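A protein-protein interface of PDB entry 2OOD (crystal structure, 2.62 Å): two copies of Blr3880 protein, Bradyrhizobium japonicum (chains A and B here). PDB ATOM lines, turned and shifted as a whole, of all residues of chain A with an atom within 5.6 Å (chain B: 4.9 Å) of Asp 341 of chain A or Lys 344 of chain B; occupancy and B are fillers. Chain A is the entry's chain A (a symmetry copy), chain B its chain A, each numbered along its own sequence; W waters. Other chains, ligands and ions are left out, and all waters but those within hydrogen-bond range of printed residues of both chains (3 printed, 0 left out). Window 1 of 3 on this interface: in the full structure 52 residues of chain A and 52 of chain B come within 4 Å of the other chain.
The side-chain carboxylate (OD1) of Asp 340 of chain B lies within hydrogen-bond range of the side-chain amide nitrogen (ND2) of Asn 331 of chain A (3.0 Å).
OD2 of Asp 340 of chain B is in salt-bridge range of NH2 of Arg 332 of chain A, at 3.3 Å.
NZ of Lys 344 of chain A is in salt-bridge range of OD2 of Asp 341 of chain B (2.8 Å).
The side-chain amino group (NZ) of Lys 344 of chain B sits at hydrogen-bond distance from the side-chain amide oxygen (OD1) of Asn 331 of chain A.
The side-chain amino group (NZ) of Lys 344 of chain B is in salt-bridge range of the side-chain carboxylate (OD2) of Asp 341 of chain A (2.8 Å).
The backbone carbonyl oxygen (O) of Met 446 of chain B sits at hydrogen-bond distance from the side-chain amide nitrogen (ND2) of Asn 331 of chain A, at 2.8 Å.
The backbone carbonyl oxygen (O) of Lys 344 of chain B lies close to the backbone carbonyl oxygen (O) of Leu 300 of chain A (3.4 Å).
OD1 of Asp 340 of chain B lies within salt-bridge range of NZ of Lys 344 of chain B (3.1 Å).
O of Lys 344 of chain B lies within hydrogen-bond range of SG of Cys 348 of chain B (3.4 Å).
OD2 of Asp 341 of chain A sits at hydrogen-bond distance from SG of Cys 297 of chain A (3.3 Å).
The side-chain carboxylate (OD1) of Asp 340 of chain A is in salt-bridge range of the side-chain amino group (NZ) of Lys 344 of chain A.
Among the printed residues, merely in contact across the chains: Phe 301 of chain A with Met 446 of chain B (3.3 Å), Gly 303 of chain A with Met 347 of chain B (3.4 Å), Phe 301 of chain A with Met 347 of chain B (3.5 Å), Phe 301 of chain A with Tyr 343 of chain B (3.5 Å), Arg 332 of chain A with Met 446 of chain B (3.5 Å), Gly 303 of chain A with Cys 348 of chain B (3.8 Å) and Leu 300 of chain A with Cys 348 of chain B (3.9 Å).
Of chain B, only Lys 344 comes within 4 Å of Asp 341 of chain A.
Of the printed residues of chain A, Lys 344 of chain B touches Leu 300, Asn 331 and Asp 341.
Printed residues of chain A within 4 Å of Tyr 343 of chain B: Phe 301.
Printed residues of chain B within 4 Å of Phe 301 of chain A: Tyr 343 (3.5 Å), Met 347 (3.5 Å) and Met 446 (3.3 Å).
Of the printed residues of chain A, Asp 341 of chain B touches Lys 344 (2.8 Å).
Of the printed residues of chain A, Asp 340 of chain B touches Asn 331 and Arg 332.
Ala 342 of chain A touches none of the printed residues of chain B.
The nearest residue of chain B that does not touch Asp 341 of chain A is Asp 341 of chain B (4.1 Å).
Printed residues of chain B that touch a printed residue of chain A: Asp 340, Asp 341, Tyr 343, Lys 344, Met 347, Cys 348 and Met 446.
Of the 18 printed residues of chain A, 7 touch a printed residue of chain B.
Printed residues of chain A that touch a printed residue of chain B: Leu 300, Phe 301, Gly 303, Asn 331, Arg 332, Asp 341 and Lys 344.
Among the printed residues, 14 pairs touch across the chains.
Among the printed residues, Asp or Glu carboxylates within 4 Å of a Lys or Arg side-chain nitrogen of the other chain: Arg 332 of chain A with Asp 340 of chain B (3.3 Å), Asp 341 of chain A with Lys 344 of chain B (2.8 Å) and Lys 344 of chain A with Asp 341 of chain B (2.8 Å).
Asp 341 of chain A touches Lys 344 of chain B, and with the chains exchanged Lys 344 of chain A touches Asp 341 of chain B.
Positions printed for both chains: 340, 341, 342, 343, 344, 345 and 346.
Of the 14 pairs that touch across the chains among the printed residues, 2 have their exchanged pair printed and touching as well.
Water W3 lies within hydrogen-bond range of OH of Tyr 343 of chain B and O of Phe 301 of chain A.
Water W2 bridges O of Cys 348 of chain B (2.8 Å) and O of Gly 303 of chain A (2.8 Å).
Water W1 lies within hydrogen-bond range of the guanidinium group of Arg 332 of chain A, the side-chain amino group of Lys 344 of chain B and the side-chain carboxylate of Asp 340 of chain B.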
ATOM      1  N   PHE A 294      28.551  17.397  -3.999  1.00  0.00           N
ATOM      2  CA  PHE A 294      28.342  16.572  -5.189  1.00  0.00           C
ATOM      3  C   PHE A 294      26.915  16.713  -5.717  1.00  0.00           C
ATOM      4  O   PHE A 294      25.974  16.218  -5.107  1.00  0.00           O
ATOM      5  CB  PHE A 294      28.673  15.110  -4.818  1.00  0.00           C
ATOM      6  CG  PHE A 294      28.357  14.088  -5.887  1.00  0.00           C
ATOM      7  CD1 PHE A 294      28.416  14.405  -7.237  1.00  0.00           C
ATOM      8  CD2 PHE A 294      28.077  12.774  -5.526  1.00  0.00           C
ATOM      9  CE1 PHE A 294      28.208  13.429  -8.209  1.00  0.00           C
ATOM     10  CE2 PHE A 294      27.868  11.789  -6.491  1.00  0.00           C
ATOM     11  CZ  PHE A 294      27.935  12.120  -7.831  1.00  0.00           C
ATOM     12  N   PRO A 296      25.185  15.554  -8.781  1.00  0.00           N
ATOM     13  CA  PRO A 296      25.074  14.726  -9.982  1.00  0.00           C
ATOM     14  C   PRO A 296      24.008  15.080 -11.012  1.00  0.00           C
ATOM     15  O   PRO A 296      24.292  15.061 -12.206  1.00  0.00           O
ATOM     16  CB  PRO A 296      24.901  13.322  -9.414  1.00  0.00           C
ATOM     17  CG  PRO A 296      24.211  13.563  -8.136  1.00  0.00           C
ATOM     18  CD  PRO A 296      24.937  14.748  -7.575  1.00  0.00           C
ATOM     19  N   CYS A 297      22.794  15.400 -10.578  1.00  0.00           N
ATOM     20  CA  CYS A 297      21.732  15.743 -11.525  1.00  0.00           C
ATOM     21  C   CYS A 297      22.112  16.938 -12.374  1.00  0.00           C
ATOM     22  O   CYS A 297      21.859  16.966 -13.576  1.00  0.00           O
ATOM     23  CB  CYS A 297      20.431  16.058 -10.797  1.00  0.00           C
ATOM     24  SG  CYS A 297      19.653  14.651 -10.030  1.00  0.00           S
ATOM     25  N   LEU A 300      25.167  16.248 -14.818  1.00  0.00           N
ATOM     26  CA  LEU A 300      24.731  15.548 -16.028  1.00  0.00           C
ATOM     27  C   LEU A 300      23.843  16.418 -16.921  1.00  0.00           C
ATOM     28  O   LEU A 300      23.993  16.424 -18.133  1.00  0.00           O
ATOM     29  CB  LEU A 300      23.983  14.256 -15.665  1.00  0.00           C
ATOM     30  CG  LEU A 300      24.755  13.175 -14.894  1.00  0.00           C
ATOM     31  CD1 LEU A 300      23.844  12.009 -14.579  1.00  0.00           C
ATOM     32  CD2 LEU A 300      25.942  12.711 -15.712  1.00  0.00           C
ATOM     33  N   PHE A 301      22.925  17.163 -16.326  1.00  0.00           N
ATOM     34  CA  PHE A 301      22.033  18.015 -17.101  1.00  0.00           C
ATOM     35  C   PHE A 301      22.782  19.100 -17.891  1.00  0.00           C
ATOM     36  O   PHE A 301      22.462  19.366 -19.054  1.00  0.00           O
ATOM     37  CB  PHE A 301      21.008  18.679 -16.171  1.00  0.00           C
ATOM     38  CG  PHE A 301      19.950  19.466 -16.895  1.00  0.00           C
ATOM     39  CD1 PHE A 301      18.819  18.835 -17.406  1.00  0.00           C
ATOM     40  CD2 PHE A 301      20.097  20.834 -17.097  1.00  0.00           C
ATOM     41  CE1 PHE A 301      17.853  19.552 -18.109  1.00  0.00           C
ATOM     42  CE2 PHE A 301      19.130  21.562 -17.805  1.00  0.00           C
ATOM     43  CZ  PHE A 301      18.010  20.914 -18.308  1.00  0.00           C
ATOM     44  N   GLY A 303      25.988  18.968 -18.611  1.00  0.00           N
ATOM     45  CA  GLY A 303      27.113  18.388 -19.316  1.00  0.00           C
ATOM     46  C   GLY A 303      28.447  18.577 -18.630  1.00  0.00           C
ATOM     47  O   GLY A 303      29.485  18.240 -19.191  1.00  0.00           O
ATOM     48  N   ASN A 331      17.577  19.015 -12.436  1.00  0.00           N
ATOM     49  CA  ASN A 331      16.159  19.012 -12.766  1.00  0.00           C
ATOM     50  C   ASN A 331      15.242  18.330 -11.763  1.00  0.00           C
ATOM     51  O   ASN A 331      14.065  18.120 -12.048  1.00  0.00           O
ATOM     52  CB  ASN A 331      15.963  18.396 -14.159  1.00  0.00           C
ATOM     53  CG  ASN A 331      16.555  16.995 -14.279  1.00  0.00           C
ATOM     54  OD1 ASN A 331      17.595  16.690 -13.696  1.00  0.00           O
ATOM     55  ND2 ASN A 331      15.901  16.143 -15.059  1.00  0.00           N
ATOM     56  N   ARG A 332      15.768  18.008 -10.585  1.00  0.00           N
ATOM     57  CA  ARG A 332      14.982  17.333  -9.551  1.00  0.00           C
ATOM     58  C   ARG A 332      15.118  18.002  -8.187  1.00  0.00           C
ATOM     59  O   ARG A 332      16.214  18.393  -7.786  1.00  0.00           O
ATOM     60  CB  ARG A 332      15.433  15.878  -9.423  1.00  0.00           C
ATOM     61  CG  ARG A 332      15.500  15.115 -10.730  1.00  0.00           C
ATOM     62  CD  ARG A 332      14.126  14.897 -11.323  1.00  0.00           C
ATOM     63  NE  ARG A 332      14.216  14.245 -12.622  1.00  0.00           N
ATOM     64  CZ  ARG A 332      13.178  14.011 -13.415  1.00  0.00           C
ATOM     65  NH1 ARG A 332      11.957  14.375 -13.041  1.00  0.00           N
ATOM     66  NH2 ARG A 332      13.366  13.424 -14.591  1.00  0.00           N
ATOM     67  N   SER A 337      16.032  11.573  -5.983  1.00  0.00           N
ATOM     68  CA  SER A 337      16.327  11.649  -7.409  1.00  0.00           C
ATOM     69  C   SER A 337      17.806  11.928  -7.600  1.00  0.00           C
ATOM     70  O   SER A 337      18.405  11.497  -8.583  1.00  0.00           O
ATOM     71  CB  SER A 337      15.518  12.762  -8.066  1.00  0.00           C
ATOM     72  OG  SER A 337      14.133  12.476  -8.034  1.00  0.00           O
ATOM     73  N   VAL A 338      18.388  12.664  -6.658  1.00  0.00           N
ATOM     74  CA  VAL A 338      19.806  12.992  -6.701  1.00  0.00           C
ATOM     75  C   VAL A 338      20.625  11.717  -6.527  1.00  0.00           C
ATOM     76  O   VAL A 338      21.648  11.541  -7.187  1.00  0.00           O
ATOM     77  CB  VAL A 338      20.194  13.989  -5.580  1.00  0.00           C
ATOM     78  CG1 VAL A 338      21.703  14.073  -5.452  1.00  0.00           C
ATOM     79  CG2 VAL A 338      19.619  15.358  -5.885  1.00  0.00           C
ATOM     80  N   LEU A 339      20.167  10.829  -5.642  1.00  0.00           N
ATOM     81  CA  LEU A 339      20.860   9.570  -5.390  1.00  0.00           C
ATOM     82  C   LEU A 339      20.821   8.669  -6.616  1.00  0.00           C
ATOM     83  O   LEU A 339      21.750   7.897  -6.849  1.00  0.00           O
ATOM     84  CB  LEU A 339      20.256   8.846  -4.177  1.00  0.00           C
ATOM     85  CG  LEU A 339      20.590   9.468  -2.811  1.00  0.00           C
ATOM     86  CD1 LEU A 339      19.787   8.799  -1.706  1.00  0.00           C
ATOM     87  CD2 LEU A 339      22.084   9.347  -2.549  1.00  0.00           C
ATOM     88  N   ASP A 340      19.751   8.772  -7.400  1.00  0.00           N
ATOM     89  CA  ASP A 340      19.610   7.978  -8.617  1.00  0.00           C
ATOM     90  C   ASP A 340      20.751   8.322  -9.579  1.00  0.00           C
ATOM     91  O   ASP A 340      21.446   7.437 -10.070  1.00  0.00           O
ATOM     92  CB  ASP A 340      18.253   8.255  -9.276  1.00  0.00           C
ATOM     93  CG  ASP A 340      18.179   7.747 -10.707  1.00  0.00           C
ATOM     94  OD1 ASP A 340      18.645   6.625 -10.974  1.00  0.00           O
ATOM     95  OD2 ASP A 340      17.642   8.463 -11.573  1.00  0.00           O
ATOM     96  N   ASP A 341      20.945   9.611  -9.840  1.00  0.00           N
ATOM     97  CA  ASP A 341      22.012  10.043 -10.730  1.00  0.00           C
ATOM     98  C   ASP A 341      23.372   9.900 -10.058  1.00  0.00           C
ATOM     99  O   ASP A 341      24.373   9.689 -10.736  1.00  0.00           O
ATOM    100  CB  ASP A 341      21.806  11.495 -11.169  1.00  0.00           C
ATOM    101  CG  ASP A 341      20.748  11.638 -12.252  1.00  0.00           C
ATOM    102  OD1 ASP A 341      20.221  10.608 -12.735  1.00  0.00           O
ATOM    103  OD2 ASP A 341      20.447  12.790 -12.629  1.00  0.00           O
ATOM    104  N   ALA A 342      23.413  10.004  -8.732  1.00  0.00           N
ATOM    105  CA  ALA A 342      24.675   9.870  -8.003  1.00  0.00           C
ATOM    106  C   ALA A 342      25.254   8.472  -8.221  1.00  0.00           C
ATOM    107  O   ALA A 342      26.448   8.306  -8.464  1.00  0.00           O
ATOM    108  CB  ALA A 342      24.456  10.123  -6.521  1.00  0.00           C
ATOM    109  N   TYR A 343      24.392   7.469  -8.128  1.00  0.00           N
ATOM    110  CA  TYR A 343      24.798   6.088  -8.332  1.00  0.00           C
ATOM    111  C   TYR A 343      25.274   5.903  -9.779  1.00  0.00           C
ATOM    112  O   TYR A 343      26.284   5.257 -10.032  1.00  0.00           O
ATOM    113  CB  TYR A 343      23.609   5.163  -8.041  1.00  0.00           C
ATOM    114  CG  TYR A 343      23.854   3.705  -8.327  1.00  0.00           C
ATOM    115  CD1 TYR A 343      24.495   2.888  -7.405  1.00  0.00           C
ATOM    116  CD2 TYR A 343      23.459   3.143  -9.531  1.00  0.00           C
ATOM    117  CE1 TYR A 343      24.740   1.534  -7.680  1.00  0.00           C
ATOM    118  CE2 TYR A 343      23.696   1.800  -9.815  1.00  0.00           C
ATOM    119  CZ  TYR A 343      24.335   1.000  -8.888  1.00  0.00           C
ATOM    120  OH  TYR A 343      24.560  -0.333  -9.179  1.00  0.00           O
ATOM    121  N   LYS A 344      24.543   6.478 -10.726  1.00  0.00           N
ATOM    122  CA  LYS A 344      24.900   6.367 -12.132  1.00  0.00           C
ATOM    123  C   LYS A 344      26.275   6.955 -12.430  1.00  0.00           C
ATOM    124  O   LYS A 344      27.062   6.358 -13.160  1.00  0.00           O
ATOM    125  CB  LYS A 344      23.823   7.030 -12.990  1.00  0.00           C
ATOM    126  CG  LYS A 344      22.525   6.251 -12.954  1.00  0.00           C
ATOM    127  CD  LYS A 344      21.386   6.910 -13.691  1.00  0.00           C
ATOM    128  CE  LYS A 344      20.173   5.994 -13.643  1.00  0.00           C
ATOM    129  NZ  LYS A 344      18.913   6.629 -14.104  1.00  0.00           N
ATOM    130  N   VAL A 345      26.572   8.121 -11.866  1.00  0.00           N
ATOM    131  CA  VAL A 345      27.875   8.749 -12.070  1.00  0.00           C
ATOM    132  C   VAL A 345      28.975   7.850 -11.498  1.00  0.00           C
ATOM    133  O   VAL A 345      30.014   7.644 -12.122  1.00  0.00           O
ATOM    134  CB  VAL A 345      27.931  10.132 -11.383  1.00  0.00           C
ATOM    135  CG1 VAL A 345      29.366  10.610 -11.265  1.00  0.00           C
ATOM    136  CG2 VAL A 345      27.113  11.118 -12.176  1.00  0.00           C
ATOM    137  N   GLY A 346      28.727   7.304 -10.312  1.00  0.00           N
ATOM    138  CA  GLY A 346      29.693   6.436  -9.672  1.00  0.00           C
ATOM    139  C   GLY A 346      29.937   5.128 -10.397  1.00  0.00           C
ATOM    140  O   GLY A 346      31.048   4.605 -10.354  1.00  0.00           O
ATOM    141  N   ASP B 340      15.014  11.664 -20.288  1.00  0.00           N
ATOM    142  CA  ASP B 340      15.695  12.458 -19.269  1.00  0.00           C
ATOM    143  C   ASP B 340      17.188  12.114 -19.276  1.00  0.00           C
ATOM    144  O   ASP B 340      18.035  12.998 -19.352  1.00  0.00           O
ATOM    145  CB  ASP B 340      15.088  12.181 -17.889  1.00  0.00           C
ATOM    146  CG  ASP B 340      15.958  12.689 -16.750  1.00  0.00           C
ATOM    147  OD1 ASP B 340      16.486  13.811 -16.849  1.00  0.00           O
ATOM    148  OD2 ASP B 340      16.109  11.973 -15.743  1.00  0.00           O
ATOM    149  N   ASP B 341      17.504  10.825 -19.202  1.00  0.00           N
ATOM    150  CA  ASP B 341      18.893  10.393 -19.215  1.00  0.00           C
ATOM    151  C   ASP B 341      19.494  10.536 -20.608  1.00  0.00           C
ATOM    152  O   ASP B 341      20.697  10.746 -20.739  1.00  0.00           O
ATOM    153  CB  ASP B 341      19.020   8.941 -18.747  1.00  0.00           C
ATOM    154  CG  ASP B 341      18.916   8.798 -17.236  1.00  0.00           C
ATOM    155  OD1 ASP B 341      18.827   9.828 -16.528  1.00  0.00           O
ATOM    156  OD2 ASP B 341      18.931   7.646 -16.754  1.00  0.00           O
ATOM    157  N   ALA B 342      18.667  10.432 -21.645  1.00  0.00           N
ATOM    158  CA  ALA B 342      19.157  10.565 -23.017  1.00  0.00           C
ATOM    159  C   ALA B 342      19.739  11.964 -23.227  1.00  0.00           C
ATOM    160  O   ALA B 342      20.807  12.130 -23.814  1.00  0.00           O
ATOM    161  CB  ALA B 342      18.030  10.313 -24.005  1.00  0.00           C
ATOM    162  N   TYR B 343      19.022  12.967 -22.739  1.00  0.00           N
ATOM    163  CA  TYR B 343      19.464  14.348 -22.846  1.00  0.00           C
ATOM    164  C   TYR B 343      20.763  14.533 -22.052  1.00  0.00           C
ATOM    165  O   TYR B 343      21.696  15.179 -22.513  1.00  0.00           O
ATOM    166  CB  TYR B 343      18.369  15.273 -22.298  1.00  0.00           C
ATOM    167  CG  TYR B 343      18.741  16.731 -22.239  1.00  0.00           C
ATOM    168  CD1 TYR B 343      18.633  17.548 -23.357  1.00  0.00           C
ATOM    169  CD2 TYR B 343      19.220  17.293 -21.066  1.00  0.00           C
ATOM    170  CE1 TYR B 343      18.997  18.902 -23.306  1.00  0.00           C
ATOM    171  CE2 TYR B 343      19.585  18.635 -21.003  1.00  0.00           C
ATOM    172  CZ  TYR B 343      19.472  19.436 -22.123  1.00  0.00           C
ATOM    173  OH  TYR B 343      19.831  20.769 -22.047  1.00  0.00           O
ATOM    174  N   LYS B 344      20.820  13.958 -20.857  1.00  0.00           N
ATOM    175  CA  LYS B 344      22.002  14.069 -20.018  1.00  0.00           C
ATOM    176  C   LYS B 344      23.243  13.481 -20.680  1.00  0.00           C
ATOM    177  O   LYS B 344      24.316  14.078 -20.634  1.00  0.00           O
ATOM    178  CB  LYS B 344      21.737  13.405 -18.665  1.00  0.00           C
ATOM    179  CG  LYS B 344      20.724  14.185 -17.853  1.00  0.00           C
ATOM    180  CD  LYS B 344      20.334  13.526 -16.553  1.00  0.00           C
ATOM    181  CE  LYS B 344      19.379  14.442 -15.805  1.00  0.00           C
ATOM    182  NZ  LYS B 344      18.717  13.807 -14.638  1.00  0.00           N
ATOM    183  N   VAL B 345      23.104  12.315 -21.302  1.00  0.00           N
ATOM    184  CA  VAL B 345      24.229  11.686 -21.991  1.00  0.00           C
ATOM    185  C   VAL B 345      24.697  12.586 -23.139  1.00  0.00           C
ATOM    186  O   VAL B 345      25.893  12.791 -23.336  1.00  0.00           O
ATOM    187  CB  VAL B 345      23.826  10.303 -22.550  1.00  0.00           C
ATOM    188  CG1 VAL B 345      24.843   9.825 -23.570  1.00  0.00           C
ATOM    189  CG2 VAL B 345      23.717   9.317 -21.417  1.00  0.00           C
ATOM    190  N   GLY B 346      23.740  13.131 -23.882  1.00  0.00           N
ATOM    191  CA  GLY B 346      24.062  13.999 -24.995  1.00  0.00           C
ATOM    192  C   GLY B 346      24.717  15.308 -24.601  1.00  0.00           C
ATOM    193  O   GLY B 346      25.536  15.830 -25.353  1.00  0.00           O
ATOM    194  N   MET B 347      24.361  15.853 -23.443  1.00  0.00           N
ATOM    195  CA  MET B 347      24.961  17.108 -23.011  1.00  0.00           C
ATOM    196  C   MET B 347      26.380  16.868 -22.530  1.00  0.00           C
ATOM    197  O   MET B 347      27.244  17.725 -22.693  1.00  0.00           O
ATOM    198  CB  MET B 347      24.140  17.773 -21.907  1.00  0.00           C
ATOM    199  CG  MET B 347      22.895  18.506 -22.410  1.00  0.00           C
ATOM    200  SD  MET B 347      23.243  19.781 -23.885  1.00  0.00           S
ATOM    201  CE  MET B 347      24.543  20.932 -22.982  1.00  0.00           C
ATOM    202  N   CYS B 348      26.625  15.705 -21.936  1.00  0.00           N
ATOM    203  CA  CYS B 348      27.968  15.392 -21.489  1.00  0.00           C
ATOM    204  C   CYS B 348      28.827  15.234 -22.730  1.00  0.00           C
ATOM    205  O   CYS B 348      30.008  15.560 -22.705  1.00  0.00           O
ATOM    206  CB  CYS B 348      27.985  14.107 -20.661  1.00  0.00           C
ATOM    207  SG  CYS B 348      27.273  14.291 -19.019  1.00  0.00           S
ATOM    208  N   MET B 446      12.169  16.537 -18.843  1.00  0.00           N
ATOM    209  CA  MET B 446      13.104  16.890 -17.782  1.00  0.00           C
ATOM    210  C   MET B 446      12.574  17.217 -16.390  1.00  0.00           C
ATOM    211  O   MET B 446      13.246  16.928 -15.402  1.00  0.00           O
ATOM    212  CB  MET B 446      13.980  18.054 -18.251  1.00  0.00           C
ATOM    213  CG  MET B 446      14.511  17.923 -19.668  1.00  0.00           C
ATOM    214  SD  MET B 446      15.485  16.262 -20.019  1.00  0.00           S
ATOM    215  CE  MET B 446      16.884  16.430 -18.661  1.00  0.00           C
HETATM  216  O   HOH W   1      16.703  12.794 -12.800  1.00  0.00           O
HETATM  217  O   HOH W   2      31.099  16.170 -20.205  1.00  0.00           O
HETATM  218  O   HOH W   3      21.700  21.452 -20.459  1.00  0.00           O
